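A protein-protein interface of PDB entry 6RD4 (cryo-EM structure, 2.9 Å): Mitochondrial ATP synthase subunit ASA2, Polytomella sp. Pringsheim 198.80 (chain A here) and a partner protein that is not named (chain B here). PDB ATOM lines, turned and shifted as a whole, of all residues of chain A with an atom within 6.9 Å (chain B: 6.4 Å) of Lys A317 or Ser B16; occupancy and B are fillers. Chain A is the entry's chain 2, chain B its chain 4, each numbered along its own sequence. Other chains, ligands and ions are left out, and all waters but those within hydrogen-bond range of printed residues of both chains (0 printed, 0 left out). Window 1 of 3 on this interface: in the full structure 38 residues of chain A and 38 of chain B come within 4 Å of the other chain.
NZ of Lys A317 is in hydrogen-bond range of O of Tyr B13 (3.4 Å).
OE2 of Glu A277 lies within salt-bridge range of NZ of Lys B18, at 3.9 Å.
The side-chain amino group (NZ) of Lys A317 sits at hydrogen-bond distance from the backbone carbonyl oxygen (O) of Gln B95, 2.6 Å away.
Leu B15 touches Glu A277.
Asp A312 touches Leu B12.
Ala A313 touches Leu B12.
CB of Ala A313 touches CD1 of Leu B15, 3.8 Å away.
Leu A316 touches Leu B12.
CE2 of Tyr B13 touches CD2 of Leu A316 (3.96 Å).
Ser B16 touches Lys A317 (CB to NZ, 3.8 Å).
Printed residues of chain B within 4 Å of Glu A277: Leu B15 and Lys B18.
Printed residues of chain B within 4 Å of Asp A312: Leu B12.
Lys A317 touches just these residues of chain B: Tyr B13 (3.4 Å), Ser B16 (3.8 Å) and Gln B95 (2.6 Å).
Of the printed residues of chain A, Tyr B13 touches Leu A316 (3.96 Å) and Lys A317 (3.4 Å).
Printed residues of chain A within 4 Å of Leu B15: Glu A277 and Ala A313.
Printed residues of chain A within 4 Å of Lys B18: Glu A277 (3.9 Å).
The nearest residue of chain B that does not touch Lys A317 is Gly B97 (4.1 Å).
The nearest printed residue of chain B that does not touch Leu A316 is Lys B55 (4.5 Å).
Hydrophobic or aromatic side chains of chain B that line the printed part of chain A: Leu B12, Tyr B13 and Leu B15.
Along chain B the printed residues that touch a printed residue of chain A span positions 12 to 95.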
ATOM      1  N   GLU A 277      -7.286  -4.263   2.680  1.00  0.00           N
ATOM      2  CA  GLU A 277      -7.238  -4.956   3.947  1.00  0.00           C
ATOM      3  C   GLU A 277      -8.440  -4.565   4.791  1.00  0.00           C
ATOM      4  O   GLU A 277      -9.017  -3.492   4.634  1.00  0.00           O
ATOM      5  CB  GLU A 277      -5.960  -4.604   4.699  1.00  0.00           C
ATOM      6  CG  GLU A 277      -4.689  -5.123   4.081  1.00  0.00           C
ATOM      7  CD  GLU A 277      -4.536  -6.614   4.235  1.00  0.00           C
ATOM      8  OE1 GLU A 277      -4.993  -7.152   5.262  1.00  0.00           O
ATOM      9  OE2 GLU A 277      -3.959  -7.253   3.331  1.00  0.00           O
ATOM     10  N   ASP A 312     -12.781  -6.682  16.657  1.00  0.00           N
ATOM     11  CA  ASP A 312     -12.680  -7.955  17.350  1.00  0.00           C
ATOM     12  C   ASP A 312     -11.377  -8.663  17.052  1.00  0.00           C
ATOM     13  O   ASP A 312     -10.845  -9.350  17.923  1.00  0.00           O
ATOM     14  CB  ASP A 312     -13.819  -8.882  16.975  1.00  0.00           C
ATOM     15  CG  ASP A 312     -15.136  -8.238  17.110  1.00  0.00           C
ATOM     16  OD1 ASP A 312     -15.997  -8.443  16.236  1.00  0.00           O
ATOM     17  OD2 ASP A 312     -15.305  -7.507  18.098  1.00  0.00           O
ATOM     18  N   ALA A 313     -10.860  -8.513  15.839  1.00  0.00           N
ATOM     19  CA  ALA A 313      -9.611  -9.156  15.477  1.00  0.00           C
ATOM     20  C   ALA A 313      -8.451  -8.612  16.281  1.00  0.00           C
ATOM     21  O   ALA A 313      -7.492  -9.337  16.535  1.00  0.00           O
ATOM     22  CB  ALA A 313      -9.347  -8.976  13.991  1.00  0.00           C
ATOM     23  N   ALA A 314      -8.511  -7.356  16.688  1.00  0.00           N
ATOM     24  CA  ALA A 314      -7.505  -6.840  17.594  1.00  0.00           C
ATOM     25  C   ALA A 314      -7.843  -7.114  19.045  1.00  0.00           C
ATOM     26  O   ALA A 314      -6.992  -6.903  19.910  1.00  0.00           O
ATOM     27  CB  ALA A 314      -7.318  -5.345  17.381  1.00  0.00           C
ATOM     28  N   ARG A 315      -9.065  -7.547  19.333  1.00  0.00           N
ATOM     29  CA  ARG A 315      -9.425  -7.978  20.675  1.00  0.00           C
ATOM     30  C   ARG A 315      -9.144  -9.452  20.896  1.00  0.00           C
ATOM     31  O   ARG A 315      -8.748  -9.842  21.996  1.00  0.00           O
ATOM     32  CB  ARG A 315     -10.901  -7.703  20.935  1.00  0.00           C
ATOM     33  CG  ARG A 315     -11.282  -7.814  22.370  1.00  0.00           C
ATOM     34  CD  ARG A 315     -12.757  -7.779  22.564  1.00  0.00           C
ATOM     35  NE  ARG A 315     -13.088  -8.187  23.916  1.00  0.00           N
ATOM     36  CZ  ARG A 315     -13.397  -9.427  24.259  1.00  0.00           C
ATOM     37  NH1 ARG A 315     -13.439 -10.378  23.344  1.00  0.00           N
ATOM     38  NH2 ARG A 315     -13.677  -9.715  25.517  1.00  0.00           N
ATOM     39  N   LEU A 316      -9.347 -10.276  19.871  1.00  0.00           N
ATOM     40  CA  LEU A 316      -8.949 -11.673  19.939  1.00  0.00           C
ATOM     41  C   LEU A 316      -7.447 -11.829  20.044  1.00  0.00           C
ATOM     42  O   LEU A 316      -6.963 -12.708  20.760  1.00  0.00           O
ATOM     43  CB  LEU A 316      -9.450 -12.407  18.710  1.00  0.00           C
ATOM     44  CG  LEU A 316     -10.655 -13.278  18.956  1.00  0.00           C
ATOM     45  CD1 LEU A 316     -11.135 -13.817  17.657  1.00  0.00           C
ATOM     46  CD2 LEU A 316     -10.214 -14.394  19.841  1.00  0.00           C
ATOM     47  N   LYS A 317      -6.694 -10.987  19.354  1.00  0.00           N
ATOM     48  CA  LYS A 317      -5.241 -11.048  19.369  1.00  0.00           C
ATOM     49  C   LYS A 317      -4.657 -10.026  20.323  1.00  0.00           C
ATOM     50  O   LYS A 317      -3.621  -9.426  20.044  1.00  0.00           O
ATOM     51  CB  LYS A 317      -4.701 -10.855  17.963  1.00  0.00           C
ATOM     52  CG  LYS A 317      -5.298 -11.811  16.954  1.00  0.00           C
ATOM     53  CD  LYS A 317      -4.523 -11.765  15.674  1.00  0.00           C
ATOM     54  CE  LYS A 317      -5.122 -12.664  14.636  1.00  0.00           C
ATOM     55  NZ  LYS A 317      -4.261 -12.713  13.426  1.00  0.00           N
ATOM     56  N   ARG A 318      -5.330  -9.814  21.448  1.00  0.00           N
ATOM     57  CA  ARG A 318      -4.948  -8.815  22.433  1.00  0.00           C
ATOM     58  C   ARG A 318      -3.637  -9.185  23.108  1.00  0.00           C
ATOM     59  O   ARG A 318      -3.323 -10.357  23.303  1.00  0.00           O
ATOM     60  CB  ARG A 318      -6.055  -8.677  23.473  1.00  0.00           C
ATOM     61  CG  ARG A 318      -5.965  -7.464  24.351  1.00  0.00           C
ATOM     62  CD  ARG A 318      -7.180  -7.296  25.208  1.00  0.00           C
ATOM     63  NE  ARG A 318      -8.048  -6.265  24.684  1.00  0.00           N
ATOM     64  CZ  ARG A 318      -9.357  -6.268  24.840  1.00  0.00           C
ATOM     65  NH1 ARG A 318      -9.933  -7.265  25.492  1.00  0.00           N
ATOM     66  NH2 ARG A 318     -10.090  -5.292  24.331  1.00  0.00           N
ATOM     67  N   SER A 319      -2.885  -8.158  23.500  1.00  0.00           N
ATOM     68  CA  SER A 319      -1.491  -8.277  23.896  1.00  0.00           C
ATOM     69  C   SER A 319      -1.243  -9.021  25.196  1.00  0.00           C
ATOM     70  O   SER A 319      -0.080  -9.111  25.594  1.00  0.00           O
ATOM     71  CB  SER A 319      -0.889  -6.887  24.034  1.00  0.00           C
ATOM     72  OG  SER A 319       0.372  -6.955  24.667  1.00  0.00           O
ATOM     73  N   SER A 320      -2.279  -9.427  25.932  1.00  0.00           N
ATOM     74  CA  SER A 320      -2.214 -10.166  27.201  1.00  0.00           C
ATOM     75  C   SER A 320      -1.532  -9.443  28.365  1.00  0.00           C
ATOM     76  O   SER A 320      -1.561  -9.934  29.494  1.00  0.00           O
ATOM     77  CB  SER A 320      -1.546 -11.527  27.031  1.00  0.00           C
ATOM     78  OG  SER A 320      -1.446 -12.169  28.287  1.00  0.00           O
ATOM     79  N   VAL B  11     -12.367 -16.407  10.953  1.00  0.00           N
ATOM     80  CA  VAL B  11     -12.158 -15.322  10.011  1.00  0.00           C
ATOM     81  C   VAL B  11     -11.699 -14.053  10.712  1.00  0.00           C
ATOM     82  O   VAL B  11     -11.187 -13.148  10.059  1.00  0.00           O
ATOM     83  CB  VAL B  11     -13.437 -15.100   9.185  1.00  0.00           C
ATOM     84  CG1 VAL B  11     -14.411 -14.228   9.917  1.00  0.00           C
ATOM     85  CG2 VAL B  11     -13.106 -14.542   7.835  1.00  0.00           C
ATOM     86  N   LEU B  12     -11.853 -13.960  12.032  1.00  0.00           N
ATOM     87  CA  LEU B  12     -11.222 -12.872  12.763  1.00  0.00           C
ATOM     88  C   LEU B  12      -9.749 -13.132  12.960  1.00  0.00           C
ATOM     89  O   LEU B  12      -8.971 -12.194  13.136  1.00  0.00           O
ATOM     90  CB  LEU B  12     -11.876 -12.689  14.120  1.00  0.00           C
ATOM     91  CG  LEU B  12     -13.283 -12.134  14.118  1.00  0.00           C
ATOM     92  CD1 LEU B  12     -13.838 -12.275  15.491  1.00  0.00           C
ATOM     93  CD2 LEU B  12     -13.257 -10.698  13.717  1.00  0.00           C
ATOM     94  N   TYR B  13      -9.374 -14.414  12.910  1.00  0.00           N
ATOM     95  CA  TYR B  13      -7.962 -14.835  13.099  1.00  0.00           C
ATOM     96  C   TYR B  13      -7.242 -14.893  11.746  1.00  0.00           C
ATOM     97  O   TYR B  13      -6.005 -15.050  11.744  1.00  0.00           O
ATOM     98  CB  TYR B  13      -7.900 -16.189  13.812  1.00  0.00           C
ATOM     99  CG  TYR B  13      -7.229 -16.162  15.162  1.00  0.00           C
ATOM    100  CD1 TYR B  13      -5.864 -16.368  15.286  1.00  0.00           C
ATOM    101  CD2 TYR B  13      -7.955 -15.930  16.318  1.00  0.00           C
ATOM    102  CE1 TYR B  13      -5.239 -16.345  16.522  1.00  0.00           C
ATOM    103  CE2 TYR B  13      -7.345 -15.902  17.562  1.00  0.00           C
ATOM    104  CZ  TYR B  13      -5.982 -16.111  17.664  1.00  0.00           C
ATOM    105  OH  TYR B  13      -5.374 -16.085  18.886  1.00  0.00           O
ATOM    106  N   PHE B  14      -7.981 -14.771  10.637  1.00  0.00           N
ATOM    107  CA  PHE B  14      -7.344 -14.826   9.339  1.00  0.00           C
ATOM    108  C   PHE B  14      -7.275 -13.464   8.675  1.00  0.00           C
ATOM    109  O   PHE B  14      -6.935 -13.384   7.498  1.00  0.00           O
ATOM    110  CB  PHE B  14      -8.064 -15.813   8.422  1.00  0.00           C
ATOM    111  CG  PHE B  14      -8.103 -17.230   8.931  1.00  0.00           C
ATOM    112  CD1 PHE B  14      -7.206 -17.700   9.876  1.00  0.00           C
ATOM    113  CD2 PHE B  14      -9.033 -18.106   8.426  1.00  0.00           C
ATOM    114  CE1 PHE B  14      -7.270 -18.992  10.327  1.00  0.00           C
ATOM    115  CE2 PHE B  14      -9.086 -19.406   8.871  1.00  0.00           C
ATOM    116  CZ  PHE B  14      -8.204 -19.843   9.823  1.00  0.00           C
ATOM    117  N   LEU B  15      -7.611 -12.396   9.395  1.00  0.00           N
ATOM    118  CA  LEU B  15      -7.553 -11.063   8.809  1.00  0.00           C
ATOM    119  C   LEU B  15      -6.118 -10.598   8.655  1.00  0.00           C
ATOM    120  O   LEU B  15      -5.724 -10.108   7.595  1.00  0.00           O
ATOM    121  CB  LEU B  15      -8.332 -10.070   9.662  1.00  0.00           C
ATOM    122  CG  LEU B  15      -9.844 -10.169   9.742  1.00  0.00           C
ATOM    123  CD1 LEU B  15     -10.377  -8.910  10.356  1.00  0.00           C
ATOM    124  CD2 LEU B  15     -10.448 -10.403   8.387  1.00  0.00           C
ATOM    125  N   SER B  16      -5.328 -10.713   9.711  1.00  0.00           N
ATOM    126  CA  SER B  16      -3.918 -10.372   9.629  1.00  0.00           C
ATOM    127  C   SER B  16      -3.068 -11.516   9.102  1.00  0.00           C
ATOM    128  O   SER B  16      -1.879 -11.310   8.849  1.00  0.00           O
ATOM    129  CB  SER B  16      -3.389  -9.932  10.995  1.00  0.00           C
ATOM    130  OG  SER B  16      -2.012  -9.611  10.918  1.00  0.00           O
ATOM    131  N   SER B  17      -3.637 -12.704   8.939  1.00  0.00           N
ATOM    132  CA  SER B  17      -2.950 -13.783   8.253  1.00  0.00           C
ATOM    133  C   SER B  17      -2.749 -13.453   6.781  1.00  0.00           C
ATOM    134  O   SER B  17      -3.493 -12.678   6.177  1.00  0.00           O
ATOM    135  CB  SER B  17      -3.732 -15.085   8.360  1.00  0.00           C
ATOM    136  OG  SER B  17      -3.154 -16.069   7.527  1.00  0.00           O
ATOM    137  N   LYS B  18      -1.720 -14.064   6.201  1.00  0.00           N
ATOM    138  CA  LYS B  18      -1.320 -13.742   4.842  1.00  0.00           C
ATOM    139  C   LYS B  18      -1.055 -14.967   3.979  1.00  0.00           C
ATOM    140  O   LYS B  18      -0.431 -14.830   2.925  1.00  0.00           O
ATOM    141  CB  LYS B  18      -0.087 -12.839   4.853  1.00  0.00           C
ATOM    142  CG  LYS B  18      -0.402 -11.397   5.203  1.00  0.00           C
ATOM    143  CD  LYS B  18       0.833 -10.519   5.170  1.00  0.00           C
ATOM    144  CE  LYS B  18       0.466  -9.066   5.402  1.00  0.00           C
ATOM    145  NZ  LYS B  18      -0.418  -8.535   4.330  1.00  0.00           N
ATOM    146  N   LYS B  55      -8.078 -20.445  21.328  1.00  0.00           N
ATOM    147  CA  LYS B  55      -7.016 -19.615  20.785  1.00  0.00           C
ATOM    148  C   LYS B  55      -5.828 -20.460  20.371  1.00  0.00           C
ATOM    149  O   LYS B  55      -5.190 -20.181  19.353  1.00  0.00           O
ATOM    150  CB  LYS B  55      -6.597 -18.583  21.819  1.00  0.00           C
ATOM    151  CG  LYS B  55      -5.399 -17.770  21.461  1.00  0.00           C
ATOM    152  CD  LYS B  55      -5.101 -16.751  22.514  1.00  0.00           C
ATOM    153  CE  LYS B  55      -4.028 -15.804  22.052  1.00  0.00           C
ATOM    154  NZ  LYS B  55      -3.681 -14.844  23.123  1.00  0.00           N
ATOM    155  N   VAL B  62      -3.082 -20.835  11.722  1.00  0.00           N
ATOM    156  CA  VAL B  62      -2.411 -19.747  11.038  1.00  0.00           C
ATOM    157  C   VAL B  62      -0.947 -20.127  10.957  1.00  0.00           C
ATOM    158  O   VAL B  62      -0.264 -19.825   9.977  1.00  0.00           O
ATOM    159  CB  VAL B  62      -2.637 -18.422  11.779  1.00  0.00           C
ATOM    160  CG1 VAL B  62      -1.945 -17.300  11.096  1.00  0.00           C
ATOM    161  CG2 VAL B  62      -4.082 -18.117  11.803  1.00  0.00           C
ATOM    162  N   ALA B  94       3.440 -13.188  15.024  1.00  0.00           N
ATOM    163  CA  ALA B  94       2.586 -12.018  15.144  1.00  0.00           C
ATOM    164  C   ALA B  94       1.304 -12.157  14.343  1.00  0.00           C
ATOM    165  O   ALA B  94       0.274 -11.620  14.742  1.00  0.00           O
ATOM    166  CB  ALA B  94       3.345 -10.785  14.695  1.00  0.00           C
ATOM    167  N   GLN B  95       1.336 -12.870  13.224  1.00  0.00           N
ATOM    168  CA  GLN B  95       0.125 -13.042  12.436  1.00  0.00           C
ATOM    169  C   GLN B  95      -0.834 -14.010  13.093  1.00  0.00           C
ATOM    170  O   GLN B  95      -2.043 -13.921  12.877  1.00  0.00           O
ATOM    171  CB  GLN B  95       0.459 -13.540  11.040  1.00  0.00           C
ATOM    172  CG  GLN B  95       0.907 -12.477  10.091  1.00  0.00           C
ATOM    173  CD  GLN B  95       1.740 -13.039   8.966  1.00  0.00           C
ATOM    174  OE1 GLN B  95       1.519 -14.163   8.513  1.00  0.00           O
ATOM    175  NE2 GLN B  95       2.721 -12.270   8.519  1.00  0.00           N
ATOM    176  N   ALA B  96      -0.321 -14.932  13.887  1.00  0.00           N
ATOM    177  CA  ALA B  96      -1.134 -15.941  14.535  1.00  0.00           C
ATOM    178  C   ALA B  96      -1.549 -15.558  15.937  1.00  0.00           C
ATOM    179  O   ALA B  96      -2.152 -16.373  16.627  1.00  0.00           O
ATOM    180  CB  ALA B  96      -0.389 -17.261  14.587  1.00  0.00           C
ATOM    181  N   GLY B  97      -1.206 -14.372  16.395  1.00  0.00           N
ATOM    182  CA  GLY B  97      -1.644 -13.925  17.686  1.00  0.00           C
ATOM    183  C   GLY B  97      -0.650 -14.087  18.800  1.00  0.00           C
ATOM    184  O   GLY B  97      -1.009 -13.856  19.955  1.00  0.00           O
